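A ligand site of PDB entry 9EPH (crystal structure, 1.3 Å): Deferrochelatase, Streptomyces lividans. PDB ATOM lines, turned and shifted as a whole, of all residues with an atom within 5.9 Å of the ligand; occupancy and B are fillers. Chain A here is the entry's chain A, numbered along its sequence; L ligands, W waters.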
ATOM      1  N   ASN A 186     -10.843  10.707 -12.029  1.00  0.00           N
ATOM      2  CA  ASN A 186     -11.095   9.988 -10.784  1.00  0.00           C
ATOM      3  C   ASN A 186      -9.748   9.625 -10.156  1.00  0.00           C
ATOM      4  O   ASN A 186      -8.700   9.927 -10.700  1.00  0.00           O
ATOM      5  CB  ASN A 186     -12.006   8.796 -10.999  1.00  0.00           C
ATOM      6  CG  ASN A 186     -11.434   7.828 -11.994  1.00  0.00           C
ATOM      7  OD1 ASN A 186     -10.241   7.513 -11.986  1.00  0.00           O
ATOM      8  ND2 ASN A 186     -12.266   7.389 -12.925  1.00  0.00           N
ATOM      9  N   LEU A 188      -8.312   6.843  -9.841  1.00  0.00           N
ATOM     10  CA  LEU A 188      -7.500   5.903 -10.600  1.00  0.00           C
ATOM     11  C   LEU A 188      -6.699   6.607 -11.680  1.00  0.00           C
ATOM     12  O   LEU A 188      -5.912   5.974 -12.389  1.00  0.00           O
ATOM     13  CB  LEU A 188      -8.359   4.806 -11.178  1.00  0.00           C
ATOM     14  CG  LEU A 188      -9.198   4.005 -10.208  1.00  0.00           C
ATOM     15  CD1 LEU A 188      -9.935   2.868 -10.912  1.00  0.00           C
ATOM     16  CD2 LEU A 188      -8.384   3.483  -9.052  1.00  0.00           C
ATOM     17  N   PHE A 190      -7.908   8.258 -14.407  1.00  0.00           N
ATOM     18  CA  PHE A 190      -8.546   8.322 -15.720  1.00  0.00           C
ATOM     19  C   PHE A 190      -9.604   9.398 -15.739  1.00  0.00           C
ATOM     20  O   PHE A 190     -10.319   9.597 -14.767  1.00  0.00           O
ATOM     21  CB  PHE A 190      -9.211   6.982 -16.032  1.00  0.00           C
ATOM     22  CG  PHE A 190      -8.218   5.981 -16.574  1.00  0.00           C
ATOM     23  CD1 PHE A 190      -7.333   5.303 -15.752  1.00  0.00           C
ATOM     24  CD2 PHE A 190      -8.151   5.658 -17.936  1.00  0.00           C
ATOM     25  CE1 PHE A 190      -6.419   4.396 -16.245  1.00  0.00           C
ATOM     26  CE2 PHE A 190      -7.212   4.756 -18.413  1.00  0.00           C
ATOM     27  CZ  PHE A 190      -6.360   4.125 -17.586  1.00  0.00           C
ATOM     28  N   LYS A 191      -9.759  10.043 -16.899  1.00  0.00           N
ATOM     29  CA  LYS A 191     -10.862  10.937 -17.147  1.00  0.00           C
ATOM     30  C   LYS A 191     -12.159  10.161 -16.999  1.00  0.00           C
ATOM     31  O   LYS A 191     -12.267   9.033 -17.471  1.00  0.00           O
ATOM     32  CB  LYS A 191     -10.777  11.494 -18.580  1.00  0.00           C
ATOM     33  CG  LYS A 191      -9.635  12.412 -18.831  1.00  0.00           C
ATOM     34  CD  LYS A 191      -9.549  12.843 -20.309  1.00  0.00           C
ATOM     35  CE  LYS A 191      -8.441  13.836 -20.585  1.00  0.00           C
ATOM     36  NZ  LYS A 191      -8.375  14.209 -22.020  1.00  0.00           N
ATOM     37  N   ASP A 192     -13.153  10.774 -16.375  1.00  0.00           N
ATOM     38  CA  ASP A 192     -14.419  10.127 -16.073  1.00  0.00           C
ATOM     39  C   ASP A 192     -15.494  11.142 -16.376  1.00  0.00           C
ATOM     40  O   ASP A 192     -15.589  12.183 -15.726  1.00  0.00           O
ATOM     41  CB  ASP A 192     -14.378   9.670 -14.614  1.00  0.00           C
ATOM     42  CG  ASP A 192     -15.360   8.573 -14.252  1.00  0.00           C
ATOM     43  OD1 ASP A 192     -16.305   8.284 -14.998  1.00  0.00           O
ATOM     44  OD2 ASP A 192     -15.102   7.985 -13.182  1.00  0.00           O
ATOM     45  N   GLY A 193     -16.283  10.840 -17.401  1.00  0.00           N
ATOM     46  CA  GLY A 193     -17.342  11.722 -17.824  1.00  0.00           C
ATOM     47  C   GLY A 193     -17.355  12.052 -19.306  1.00  0.00           C
ATOM     48  O   GLY A 193     -18.243  12.767 -19.730  1.00  0.00           O
ATOM     49  N   THR A 194     -16.443  11.494 -20.117  1.00  0.00           N
ATOM     50  CA  THR A 194     -16.395  11.843 -21.518  1.00  0.00           C
ATOM     51  C   THR A 194     -17.711  11.574 -22.221  1.00  0.00           C
ATOM     52  O   THR A 194     -18.216  12.436 -22.945  1.00  0.00           O
ATOM     53  CB  THR A 194     -15.250  11.060 -22.132  1.00  0.00           C
ATOM     54  OG1 THR A 194     -14.032  11.334 -21.459  1.00  0.00           O
ATOM     55  CG2 THR A 194     -15.144  11.346 -23.608  1.00  0.00           C
ATOM     56  N   ARG A 195     -18.231  10.343 -22.121  1.00  0.00           N
ATOM     57  CA  ARG A 195     -19.447   9.954 -22.803  1.00  0.00           C
ATOM     58  C   ARG A 195     -20.592   9.878 -21.806  1.00  0.00           C
ATOM     59  O   ARG A 195     -20.940   8.817 -21.308  1.00  0.00           O
ATOM     60  CB  ARG A 195     -19.264   8.662 -23.591  1.00  0.00           C
ATOM     61  CG  ARG A 195     -18.615   8.895 -24.951  1.00  0.00           C
ATOM     62  CD  ARG A 195     -18.398   7.687 -25.787  1.00  0.00           C
ATOM     63  NE  ARG A 195     -19.516   6.764 -25.758  1.00  0.00           N
ATOM     64  CZ  ARG A 195     -20.715   7.016 -26.240  1.00  0.00           C
ATOM     65  NH1 ARG A 195     -21.686   6.282 -25.795  1.00  0.00           N
ATOM     66  NH2 ARG A 195     -20.942   7.940 -27.158  1.00  0.00           N
ATOM     67  N   ASN A 196     -21.115  11.042 -21.460  1.00  0.00           N
ATOM     68  CA  ASN A 196     -22.215  11.182 -20.553  1.00  0.00           C
ATOM     69  C   ASN A 196     -23.413  11.734 -21.345  1.00  0.00           C
ATOM     70  O   ASN A 196     -23.644  11.311 -22.479  1.00  0.00           O
ATOM     71  CB  ASN A 196     -21.735  11.936 -19.314  1.00  0.00           C
ATOM     72  CG  ASN A 196     -22.650  11.783 -18.146  1.00  0.00           C
ATOM     73  OD1 ASN A 196     -23.226  10.711 -17.939  1.00  0.00           O
ATOM     74  ND2 ASN A 196     -22.813  12.814 -17.365  1.00  0.00           N
ATOM     75  N   ARG A 229     -24.226   4.781  -5.279  1.00  0.00           N
ATOM     76  CA  ARG A 229     -23.426   3.640  -4.868  1.00  0.00           C
ATOM     77  C   ARG A 229     -22.117   4.143  -4.319  1.00  0.00           C
ATOM     78  O   ARG A 229     -21.395   4.904  -4.979  1.00  0.00           O
ATOM     79  CB  ARG A 229     -23.113   2.710  -6.040  1.00  0.00           C
ATOM     80  CG  ARG A 229     -24.320   2.105  -6.716  1.00  0.00           C
ATOM     81  CD  ARG A 229     -25.093   1.076  -5.903  1.00  0.00           C
ATOM     82  NE  ARG A 229     -24.314  -0.173  -5.953  1.00  0.00           N
ATOM     83  CZ  ARG A 229     -24.791  -1.361  -5.683  1.00  0.00           C
ATOM     84  NH1 ARG A 229     -26.004  -1.516  -5.196  1.00  0.00           N
ATOM     85  NH2 ARG A 229     -24.010  -2.414  -5.865  1.00  0.00           N
ATOM     86  N   ILE A 231     -18.464   3.375  -3.587  1.00  0.00           N
ATOM     87  CA  ILE A 231     -17.543   2.398  -4.143  1.00  0.00           C
ATOM     88  C   ILE A 231     -16.158   2.654  -3.593  1.00  0.00           C
ATOM     89  O   ILE A 231     -15.566   3.692  -3.845  1.00  0.00           O
ATOM     90  CB  ILE A 231     -17.545   2.466  -5.674  1.00  0.00           C
ATOM     91  CG1 ILE A 231     -18.959   2.316  -6.193  1.00  0.00           C
ATOM     92  CG2 ILE A 231     -16.653   1.360  -6.276  1.00  0.00           C
ATOM     93  CD1 ILE A 231     -19.124   2.443  -7.713  1.00  0.00           C
ATOM     94  N   MET A 233     -12.212   1.981  -3.645  1.00  0.00           N
ATOM     95  CA  MET A 233     -11.190   1.632  -4.627  1.00  0.00           C
ATOM     96  C   MET A 233     -10.015   0.984  -3.920  1.00  0.00           C
ATOM     97  O   MET A 233      -9.542   1.485  -2.921  1.00  0.00           O
ATOM     98  CB  MET A 233     -10.681   2.898  -5.342  1.00  0.00           C
ATOM     99  CG  MET A 233     -11.701   3.465  -6.282  1.00  0.00           C
ATOM    100  SD  MET A 233     -11.185   5.139  -6.777  1.00  0.00           S
ATOM    101  CE  MET A 233     -12.111   5.357  -8.294  1.00  0.00           C
ATOM    102  N   PHE A 250      -9.930  -0.288 -18.845  1.00  0.00           N
ATOM    103  CA  PHE A 250     -10.917   0.676 -19.281  1.00  0.00           C
ATOM    104  C   PHE A 250     -11.260   0.621 -20.776  1.00  0.00           C
ATOM    105  O   PHE A 250     -12.416   0.805 -21.148  1.00  0.00           O
ATOM    106  CB  PHE A 250     -10.515   2.107 -18.908  1.00  0.00           C
ATOM    107  CG  PHE A 250     -10.728   2.323 -17.430  1.00  0.00           C
ATOM    108  CD1 PHE A 250     -12.018   2.351 -16.948  1.00  0.00           C
ATOM    109  CD2 PHE A 250      -9.680   2.506 -16.557  1.00  0.00           C
ATOM    110  CE1 PHE A 250     -12.261   2.483 -15.598  1.00  0.00           C
ATOM    111  CE2 PHE A 250      -9.936   2.684 -15.206  1.00  0.00           C
ATOM    112  CZ  PHE A 250     -11.220   2.651 -14.752  1.00  0.00           C
ATOM    113  N   ARG A 252      -9.558   2.774 -22.758  1.00  0.00           N
ATOM    114  CA  ARG A 252      -9.113   4.095 -23.135  1.00  0.00           C
ATOM    115  C   ARG A 252      -7.700   4.252 -22.623  1.00  0.00           C
ATOM    116  O   ARG A 252      -7.344   3.615 -21.645  1.00  0.00           O
ATOM    117  CB  ARG A 252      -9.977   5.209 -22.554  1.00  0.00           C
ATOM    118  CG  ARG A 252     -11.343   5.280 -23.202  1.00  0.00           C
ATOM    119  CD  ARG A 252     -12.231   6.308 -22.576  1.00  0.00           C
ATOM    120  NE  ARG A 252     -13.520   6.481 -23.231  1.00  0.00           N
ATOM    121  CZ  ARG A 252     -13.793   7.328 -24.214  1.00  0.00           C
ATOM    122  NH1 ARG A 252     -12.858   8.083 -24.746  1.00  0.00           N
ATOM    123  NH2 ARG A 252     -15.047   7.444 -24.613  1.00  0.00           N
ATOM    124  N   PRO A 269     -15.665   5.508 -29.473  1.00  0.00           N
ATOM    125  CA  PRO A 269     -15.087   4.205 -29.260  1.00  0.00           C
ATOM    126  C   PRO A 269     -15.380   3.233 -30.386  1.00  0.00           C
ATOM    127  O   PRO A 269     -16.497   3.244 -30.890  1.00  0.00           O
ATOM    128  CB  PRO A 269     -15.716   3.684 -27.986  1.00  0.00           C
ATOM    129  CG  PRO A 269     -16.648   4.733 -27.539  1.00  0.00           C
ATOM    130  CD  PRO A 269     -16.610   5.964 -28.454  1.00  0.00           C
ATOM    131  N   HIS A 279     -14.124  -2.029 -19.186  1.00  0.00           N
ATOM    132  CA  HIS A 279     -15.239  -1.301 -18.584  1.00  0.00           C
ATOM    133  C   HIS A 279     -16.067  -0.560 -19.624  1.00  0.00           C
ATOM    134  O   HIS A 279     -17.283  -0.603 -19.576  1.00  0.00           O
ATOM    135  CB  HIS A 279     -14.676  -0.391 -17.507  1.00  0.00           C
ATOM    136  CG  HIS A 279     -15.698   0.416 -16.813  1.00  0.00           C
ATOM    137  ND1 HIS A 279     -16.553  -0.092 -15.889  1.00  0.00           N
ATOM    138  CD2 HIS A 279     -15.993   1.741 -16.878  1.00  0.00           C
ATOM    139  CE1 HIS A 279     -17.328   0.900 -15.437  1.00  0.00           C
ATOM    140  NE2 HIS A 279     -17.029   2.019 -16.014  1.00  0.00           N
ATOM    141  N   VAL A 280     -15.411   0.214 -20.509  1.00  0.00           N
ATOM    142  CA  VAL A 280     -16.167   0.993 -21.479  1.00  0.00           C
ATOM    143  C   VAL A 280     -16.966   0.084 -22.404  1.00  0.00           C
ATOM    144  O   VAL A 280     -18.102   0.424 -22.744  1.00  0.00           O
ATOM    145  CB  VAL A 280     -15.231   1.938 -22.244  1.00  0.00           C
ATOM    146  CG1 VAL A 280     -15.917   2.554 -23.447  1.00  0.00           C
ATOM    147  CG2 VAL A 280     -14.665   3.008 -21.319  1.00  0.00           C
ATOM    148  N   ALA A 283     -19.995  -1.151 -20.470  1.00  0.00           N
ATOM    149  CA  ALA A 283     -20.927  -0.143 -19.993  1.00  0.00           C
ATOM    150  C   ALA A 283     -21.568   0.645 -21.111  1.00  0.00           C
ATOM    151  O   ALA A 283     -22.523   1.360 -20.869  1.00  0.00           O
ATOM    152  CB  ALA A 283     -20.173   0.808 -19.067  1.00  0.00           C
ATOM    153  N   HIS A 284     -21.043   0.575 -22.345  1.00  0.00           N
ATOM    154  CA  HIS A 284     -21.493   1.424 -23.435  1.00  0.00           C
ATOM    155  C   HIS A 284     -22.941   1.108 -23.752  1.00  0.00           C
ATOM    156  O   HIS A 284     -23.331  -0.049 -23.675  1.00  0.00           O
ATOM    157  CB  HIS A 284     -20.631   1.108 -24.658  1.00  0.00           C
ATOM    158  CG  HIS A 284     -20.743   2.044 -25.775  1.00  0.00           C
ATOM    159  ND1 HIS A 284     -21.788   2.038 -26.663  1.00  0.00           N
ATOM    160  CD2 HIS A 284     -19.918   3.052 -26.178  1.00  0.00           C
ATOM    161  CE1 HIS A 284     -21.589   2.998 -27.551  1.00  0.00           C
ATOM    162  NE2 HIS A 284     -20.440   3.615 -27.306  1.00  0.00           N
ATOM    163  N   PRO A 285     -23.748   2.107 -24.141  1.00  0.00           N
ATOM    164  CA  PRO A 285     -25.147   1.852 -24.514  1.00  0.00           C
ATOM    165  C   PRO A 285     -25.319   0.755 -25.560  1.00  0.00           C
ATOM    166  O   PRO A 285     -26.269  -0.027 -25.429  1.00  0.00           O
ATOM    167  CB  PRO A 285     -25.577   3.204 -25.044  1.00  0.00           C
ATOM    168  CG  PRO A 285     -24.811   4.177 -24.180  1.00  0.00           C
ATOM    169  CD  PRO A 285     -23.453   3.535 -24.128  1.00  0.00           C
ATOM    170  N   LEU A 293     -27.165   6.446 -19.146  1.00  0.00           N
ATOM    171  CA  LEU A 293     -27.303   7.034 -17.823  1.00  0.00           C
ATOM    172  C   LEU A 293     -26.738   8.429 -17.832  1.00  0.00           C
ATOM    173  O   LEU A 293     -25.868   8.723 -18.627  1.00  0.00           O
ATOM    174  CB  LEU A 293     -26.403   6.249 -16.855  1.00  0.00           C
ATOM    175  CG  LEU A 293     -26.640   4.759 -16.740  1.00  0.00           C
ATOM    176  CD1 LEU A 293     -25.606   4.147 -15.801  1.00  0.00           C
ATOM    177  CD2 LEU A 293     -28.039   4.517 -16.238  1.00  0.00           C
ATOM    178  N   ARG A 295     -24.388  10.204 -15.427  1.00  0.00           N
ATOM    179  CA  ARG A 295     -23.515   9.979 -14.303  1.00  0.00           C
ATOM    180  C   ARG A 295     -23.111  11.305 -13.702  1.00  0.00           C
ATOM    181  O   ARG A 295     -22.804  12.246 -14.453  1.00  0.00           O
ATOM    182  CB  ARG A 295     -22.260   9.241 -14.775  1.00  0.00           C
ATOM    183  CG  ARG A 295     -22.570   7.814 -15.205  1.00  0.00           C
ATOM    184  CD  ARG A 295     -21.365   7.171 -15.736  1.00  0.00           C
ATOM    185  NE  ARG A 295     -21.056   7.691 -17.056  1.00  0.00           N
ATOM    186  CZ  ARG A 295     -19.853   7.955 -17.524  1.00  0.00           C
ATOM    187  NH1 ARG A 295     -18.759   7.783 -16.812  1.00  0.00           N
ATOM    188  NH2 ARG A 295     -19.711   8.411 -18.755  1.00  0.00           N
ATOM    189  N   LEU A 314     -15.140   6.341  -4.790  1.00  0.00           N
ATOM    190  CA  LEU A 314     -15.961   7.096  -5.709  1.00  0.00           C
ATOM    191  C   LEU A 314     -17.396   6.942  -5.246  1.00  0.00           C
ATOM    192  O   LEU A 314     -17.874   5.836  -5.037  1.00  0.00           O
ATOM    193  CB  LEU A 314     -15.706   6.592  -7.126  1.00  0.00           C
ATOM    194  CG  LEU A 314     -16.214   7.491  -8.234  1.00  0.00           C
ATOM    195  CD1 LEU A 314     -15.417   7.369  -9.467  1.00  0.00           C
ATOM    196  CD2 LEU A 314     -17.637   7.214  -8.558  1.00  0.00           C
ATOM    197  N   PHE A 316     -20.692   7.152  -6.575  1.00  0.00           N
ATOM    198  CA  PHE A 316     -21.279   7.080  -7.893  1.00  0.00           C
ATOM    199  C   PHE A 316     -22.742   7.454  -7.801  1.00  0.00           C
ATOM    200  O   PHE A 316     -23.469   6.934  -6.992  1.00  0.00           O
ATOM    201  CB  PHE A 316     -21.158   5.620  -8.356  1.00  0.00           C
ATOM    202  CG  PHE A 316     -21.703   5.400  -9.757  1.00  0.00           C
ATOM    203  CD1 PHE A 316     -20.880   5.643 -10.836  1.00  0.00           C
ATOM    204  CD2 PHE A 316     -22.999   4.998  -9.972  1.00  0.00           C
ATOM    205  CE1 PHE A 316     -21.371   5.445 -12.141  1.00  0.00           C
ATOM    206  CE2 PHE A 316     -23.471   4.840 -11.268  1.00  0.00           C
ATOM    207  CZ  PHE A 316     -22.627   5.054 -12.322  1.00  0.00           C
ATOM    208  N   PHE A 327     -29.681   1.948 -14.649  1.00  0.00           N
ATOM    209  CA  PHE A 327     -28.593   1.381 -13.876  1.00  0.00           C
ATOM    210  C   PHE A 327     -28.613  -0.145 -13.835  1.00  0.00           C
ATOM    211  O   PHE A 327     -27.558  -0.756 -13.922  1.00  0.00           O
ATOM    212  CB  PHE A 327     -28.665   1.931 -12.457  1.00  0.00           C
ATOM    213  CG  PHE A 327     -27.628   1.391 -11.507  1.00  0.00           C
ATOM    214  CD1 PHE A 327     -26.330   1.892 -11.499  1.00  0.00           C
ATOM    215  CD2 PHE A 327     -27.895   0.306 -10.701  1.00  0.00           C
ATOM    216  CE1 PHE A 327     -25.363   1.396 -10.667  1.00  0.00           C
ATOM    217  CE2 PHE A 327     -26.905  -0.192  -9.858  1.00  0.00           C
ATOM    218  CZ  PHE A 327     -25.652   0.313  -9.870  1.00  0.00           C
ATOM    219  N   VAL A 330     -27.077  -1.986 -16.928  1.00  0.00           N
ATOM    220  CA  VAL A 330     -25.686  -1.692 -17.112  1.00  0.00           C
ATOM    221  C   VAL A 330     -24.867  -2.339 -15.988  1.00  0.00           C
ATOM    222  O   VAL A 330     -23.881  -3.004 -16.267  1.00  0.00           O
ATOM    223  CB  VAL A 330     -25.491  -0.172 -17.198  1.00  0.00           C
ATOM    224  CG1 VAL A 330     -24.014   0.153 -17.293  1.00  0.00           C
ATOM    225  CG2 VAL A 330     -26.235   0.432 -18.380  1.00  0.00           C
ATOM    226  N   GLN A 331     -25.298  -2.223 -14.733  1.00  0.00           N
ATOM    227  CA  GLN A 331     -24.554  -2.878 -13.664  1.00  0.00           C
ATOM    228  C   GLN A 331     -24.544  -4.395 -13.833  1.00  0.00           C
ATOM    229  O   GLN A 331     -23.545  -5.027 -13.530  1.00  0.00           O
ATOM    230  CB  GLN A 331     -25.081  -2.449 -12.308  1.00  0.00           C
ATOM    231  CG  GLN A 331     -24.387  -3.022 -11.094  1.00  0.00           C
ATOM    232  CD  GLN A 331     -22.924  -2.706 -10.955  1.00  0.00           C
ATOM    233  OE1 GLN A 331     -22.472  -1.622 -11.317  1.00  0.00           O
ATOM    234  NE2 GLN A 331     -22.156  -3.618 -10.416  1.00  0.00           N
ATOM    235  N   LEU A 334     -21.844  -5.402 -15.933  1.00  0.00           N
ATOM    236  CA  LEU A 334     -20.518  -5.208 -15.367  1.00  0.00           C
ATOM    237  C   LEU A 334     -20.103  -6.390 -14.494  1.00  0.00           C
ATOM    238  O   LEU A 334     -19.052  -6.340 -13.862  1.00  0.00           O
ATOM    239  CB  LEU A 334     -20.400  -3.901 -14.587  1.00  0.00           C
ATOM    240  CG  LEU A 334     -20.653  -2.653 -15.425  1.00  0.00           C
ATOM    241  CD1 LEU A 334     -20.466  -1.380 -14.586  1.00  0.00           C
ATOM    242  CD2 LEU A 334     -19.777  -2.525 -16.613  1.00  0.00           C
ATOM    243  N   LEU A 339     -12.626  -4.067 -14.159  1.00  0.00           N
ATOM    244  CA  LEU A 339     -12.548  -3.097 -13.073  1.00  0.00           C
ATOM    245  C   LEU A 339     -12.936  -3.697 -11.725  1.00  0.00           C
ATOM    246  O   LEU A 339     -12.479  -3.233 -10.678  1.00  0.00           O
ATOM    247  CB  LEU A 339     -13.424  -1.891 -13.405  1.00  0.00           C
ATOM    248  CG  LEU A 339     -13.406  -0.745 -12.387  1.00  0.00           C
ATOM    249  CD1 LEU A 339     -12.016  -0.142 -12.265  1.00  0.00           C
ATOM    250  CD2 LEU A 339     -14.442   0.277 -12.807  1.00  0.00           C
ATOM    251  N   ILE A 343     -12.334  -2.619  -7.195  1.00  0.00           N
ATOM    252  CA  ILE A 343     -13.378  -1.833  -6.545  1.00  0.00           C
ATOM    253  C   ILE A 343     -14.271  -2.767  -5.732  1.00  0.00           C
ATOM    254  O   ILE A 343     -14.282  -3.975  -5.932  1.00  0.00           O
ATOM    255  CB  ILE A 343     -14.235  -1.051  -7.559  1.00  0.00           C
ATOM    256  CG1 ILE A 343     -15.036  -1.980  -8.475  1.00  0.00           C
ATOM    257  CG2 ILE A 343     -13.360  -0.077  -8.334  1.00  0.00           C
ATOM    258  CD1 ILE A 343     -16.152  -1.279  -9.233  1.00  0.00           C
ATOM    259  N   HIS A 345     -18.394  -2.305  -4.104  1.00  0.00           N
ATOM    260  CA  HIS A 345     -19.528  -1.482  -3.713  1.00  0.00           C
ATOM    261  C   HIS A 345     -19.853  -1.760  -2.254  1.00  0.00           C
ATOM    262  O   HIS A 345     -20.080  -2.919  -1.895  1.00  0.00           O
ATOM    263  CB  HIS A 345     -20.705  -1.827  -4.587  1.00  0.00           C
ATOM    264  CG  HIS A 345     -20.561  -1.486  -6.016  1.00  0.00           C
ATOM    265  ND1 HIS A 345     -21.539  -0.737  -6.647  1.00  0.00           N
ATOM    266  CD2 HIS A 345     -19.657  -1.773  -6.960  1.00  0.00           C
ATOM    267  CE1 HIS A 345     -21.187  -0.600  -7.924  1.00  0.00           C
ATOM    268  NE2 HIS A 345     -20.063  -1.259  -8.140  1.00  0.00           N
HETATM  269  C1  LIG L   1     -17.274   5.192 -18.515  1.00  0.00           C
HETATM  270  C2  LIG L   1     -14.488   4.783 -14.605  1.00  0.00           C
HETATM  271  C3  LIG L   1     -18.184   2.825 -12.169  1.00  0.00           C
HETATM  272  C4  LIG L   1     -20.929   3.320 -16.100  1.00  0.00           C
HETATM  273  C5  LIG L   1     -16.164   5.234 -17.693  1.00  0.00           C
HETATM  274  C6  LIG L   1     -14.901   5.741 -18.054  1.00  0.00           C
HETATM  275  C7  LIG L   1     -14.081   5.621 -16.967  1.00  0.00           C
HETATM  276  C8  LIG L   1     -14.879   5.056 -15.922  1.00  0.00           C
HETATM  277  C9  LIG L   1     -12.641   5.969 -16.809  1.00  0.00           C
HETATM  278  C10 LIG L   1     -14.468   6.254 -19.416  1.00  0.00           C
HETATM  279  C11 LIG L   1     -14.760   7.742 -19.684  1.00  0.00           C
HETATM  280  C12 LIG L   1     -16.211   8.068 -19.745  1.00  0.00           C
HETATM  281  O1  LIG L   1     -16.786   8.495 -18.712  1.00  0.00           O
HETATM  282  O2  LIG L   1     -16.854   7.979 -20.819  1.00  0.00           O
HETATM  283  C13 LIG L   1     -15.285   4.215 -13.604  1.00  0.00           C
HETATM  284  C14 LIG L   1     -14.794   3.979 -12.274  1.00  0.00           C
HETATM  285  C15 LIG L   1     -15.819   3.441 -11.594  1.00  0.00           C
HETATM  286  C16 LIG L   1     -16.949   3.316 -12.502  1.00  0.00           C
HETATM  287  C17 LIG L   1     -13.412   4.275 -11.768  1.00  0.00           C
HETATM  288  C18 LIG L   1     -15.961   3.012 -10.190  1.00  0.00           C
HETATM  289  C19 LIG L   1     -15.143   3.316  -9.273  1.00  0.00           C
HETATM  290  C20 LIG L   1     -19.263   2.762 -13.026  1.00  0.00           C
HETATM  291  C21 LIG L   1     -20.517   2.198 -12.730  1.00  0.00           C
HETATM  292  C22 LIG L   1     -21.307   2.342 -13.839  1.00  0.00           C
HETATM  293  C23 LIG L   1     -20.494   2.943 -14.838  1.00  0.00           C
HETATM  294  C24 LIG L   1     -20.926   1.666 -11.387  1.00  0.00           C
HETATM  295  C25 LIG L   1     -22.699   1.952 -14.078  1.00  0.00           C
HETATM  296  C26 LIG L   1     -23.336   1.031 -13.488  1.00  0.00           C
HETATM  297  C27 LIG L   1     -20.152   3.965 -17.056  1.00  0.00           C
HETATM  298  C28 LIG L   1     -20.687   4.359 -18.362  1.00  0.00           C
HETATM  299  C29 LIG L   1     -19.674   4.861 -19.074  1.00  0.00           C
HETATM  300  C30 LIG L   1     -18.510   4.751 -18.177  1.00  0.00           C
HETATM  301  C31 LIG L   1     -22.113   4.231 -18.808  1.00  0.00           C
HETATM  302  C32 LIG L   1     -19.728   5.391 -20.454  1.00  0.00           C
HETATM  303  C33 LIG L   1     -19.562   4.285 -21.558  1.00  0.00           C
HETATM  304  C34 LIG L   1     -19.693   4.826 -22.921  1.00  0.00           C
HETATM  305  O3  LIG L   1     -18.671   5.079 -23.603  1.00  0.00           O
HETATM  306  O4  LIG L   1     -20.843   5.123 -23.300  1.00  0.00           O
HETATM  307  N1  LIG L   1     -16.138   4.835 -16.342  1.00  0.00           N
HETATM  308  N2  LIG L   1     -16.551   3.826 -13.689  1.00  0.00           N
HETATM  309  N3  LIG L   1     -19.263   3.183 -14.319  1.00  0.00           N
HETATM  310  N4  LIG L   1     -18.844   4.233 -16.975  1.00  0.00           N
HETATM  311 FE1  LIG L   1     -17.672   3.928 -15.406  1.00  0.00          FE
HETATM  312  O   HOH W   1     -24.743   3.108 -20.564  1.00  0.00           O
HETATM  313  O   HOH W   2     -18.017   6.078 -14.641  1.00  0.00           O
HETATM  314  O   HOH W   3     -24.593   5.859 -20.439  1.00  0.00           O
HETATM  315  O   HOH W   4     -16.345   5.982 -22.589  1.00  0.00           O
HETATM  316  O   HOH W   5     -17.199   6.729 -12.116  1.00  0.00           O
HETATM  317  O   HOH W   6     -22.703   6.863 -22.312  1.00  0.00           O
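Water W2 lies within hydrogen-bond range of the side-chain carboxylate (OD1) of Asp 192 (2.8 Å) and the guanidinium group (NH1) of Arg 295 (2.9 Å).
Water W4 lies within hydrogen-bond range of O3 of the ligand (2.7 Å) and NH2 of Arg 252 (2.8 Å).
Water W6 lies within hydrogen-bond range of an oxygen (O4) of the ligand and the backbone carbonyl oxygen of Arg 195.
An iron atom (FE1) of the ligand is bound by a ring nitrogen (NE2) of His 279 (2.1 Å).
An oxygen (O1) of the ligand lies within hydrogen-bond range of the backbone NH of Gly 193 (2.7 Å).
An oxygen (O1) of the ligand lies within salt-bridge range of the guanidinium group of Arg 295 (2.8 Å).
The backbone NH (N) of Arg 195 is in hydrogen-bond range of an oxygen (O2) of the ligand, at 3.0 Å.
An oxygen (O3) of the ligand is in salt-bridge range of the guanidinium group (NE) of Arg 195, at 2.9 Å.
N of Thr 194 sits at hydrogen-bond distance from O1 of the ligand (3.3 Å).
Residues that only touch the ligand: Lys 191 (3.2 Å), Pro 285 (3.2 Å), Phe 250 (3.4 Å), Phe 316 (3.4 Å), Phe 327 (3.5 Å), His 284 (3.5 Å), Asn 186 (3.5 Å), Gln 331 (3.5 Å), Asp 192 (3.6 Å), Ala 283 (3.6 Å), Leu 339 (3.7 Å), Phe 190 (3.7 Å), Val 280 (3.7 Å), Met 233 (3.8 Å), Leu 188 (3.8 Å), Arg 252 (3.9 Å), Ile 231 (3.9 Å), Leu 334 (3.9 Å), Val 330 (3.9 Å), Ile 343 (3.9 Å) and Leu 314 (3.96 Å).
Hydrophobic or aromatic side chains that line the ligand: Leu 188, Phe 190, Ile 231, Met 233, Phe 250, His 279, Val 280, Ala 283, His 284, Pro 285, Leu 314, Phe 316, Phe 327, Val 330, Leu 334, Leu 339 and Ile 343.
Of the 31 residues printed, 26 come within 4 Å of the ligand.
The nearest printed residue that does not touch the ligand is Leu 293 (4.03 Å).
NH2 of Arg 295 lies within hydrogen-bond range of O of Arg 195.
NH1 of Arg 295 is in salt-bridge range of OD1 of Asp 192 (3.1 Å).
The side-chain amide oxygen (OD1) of Asn 196 lies within hydrogen-bond range of the backbone NH (N) of Arg 295 (2.8 Å).
O of Phe 250 is in hydrogen-bond range of N of Val 280.
The backbone carbonyl oxygen of Arg 229 is in hydrogen-bond range of the backbone NH of Phe 316, at 2.8 Å.
OD2 of Asp 192 sits at hydrogen-bond distance from ND2 of Asn 186.
OD1 of Asn 186 lies within hydrogen-bond range of N of Leu 188, 3.0 Å away.
The backbone carbonyl oxygen of Ile 231 lies within hydrogen-bond range of the backbone NH of Leu 314 (2.8 Å).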
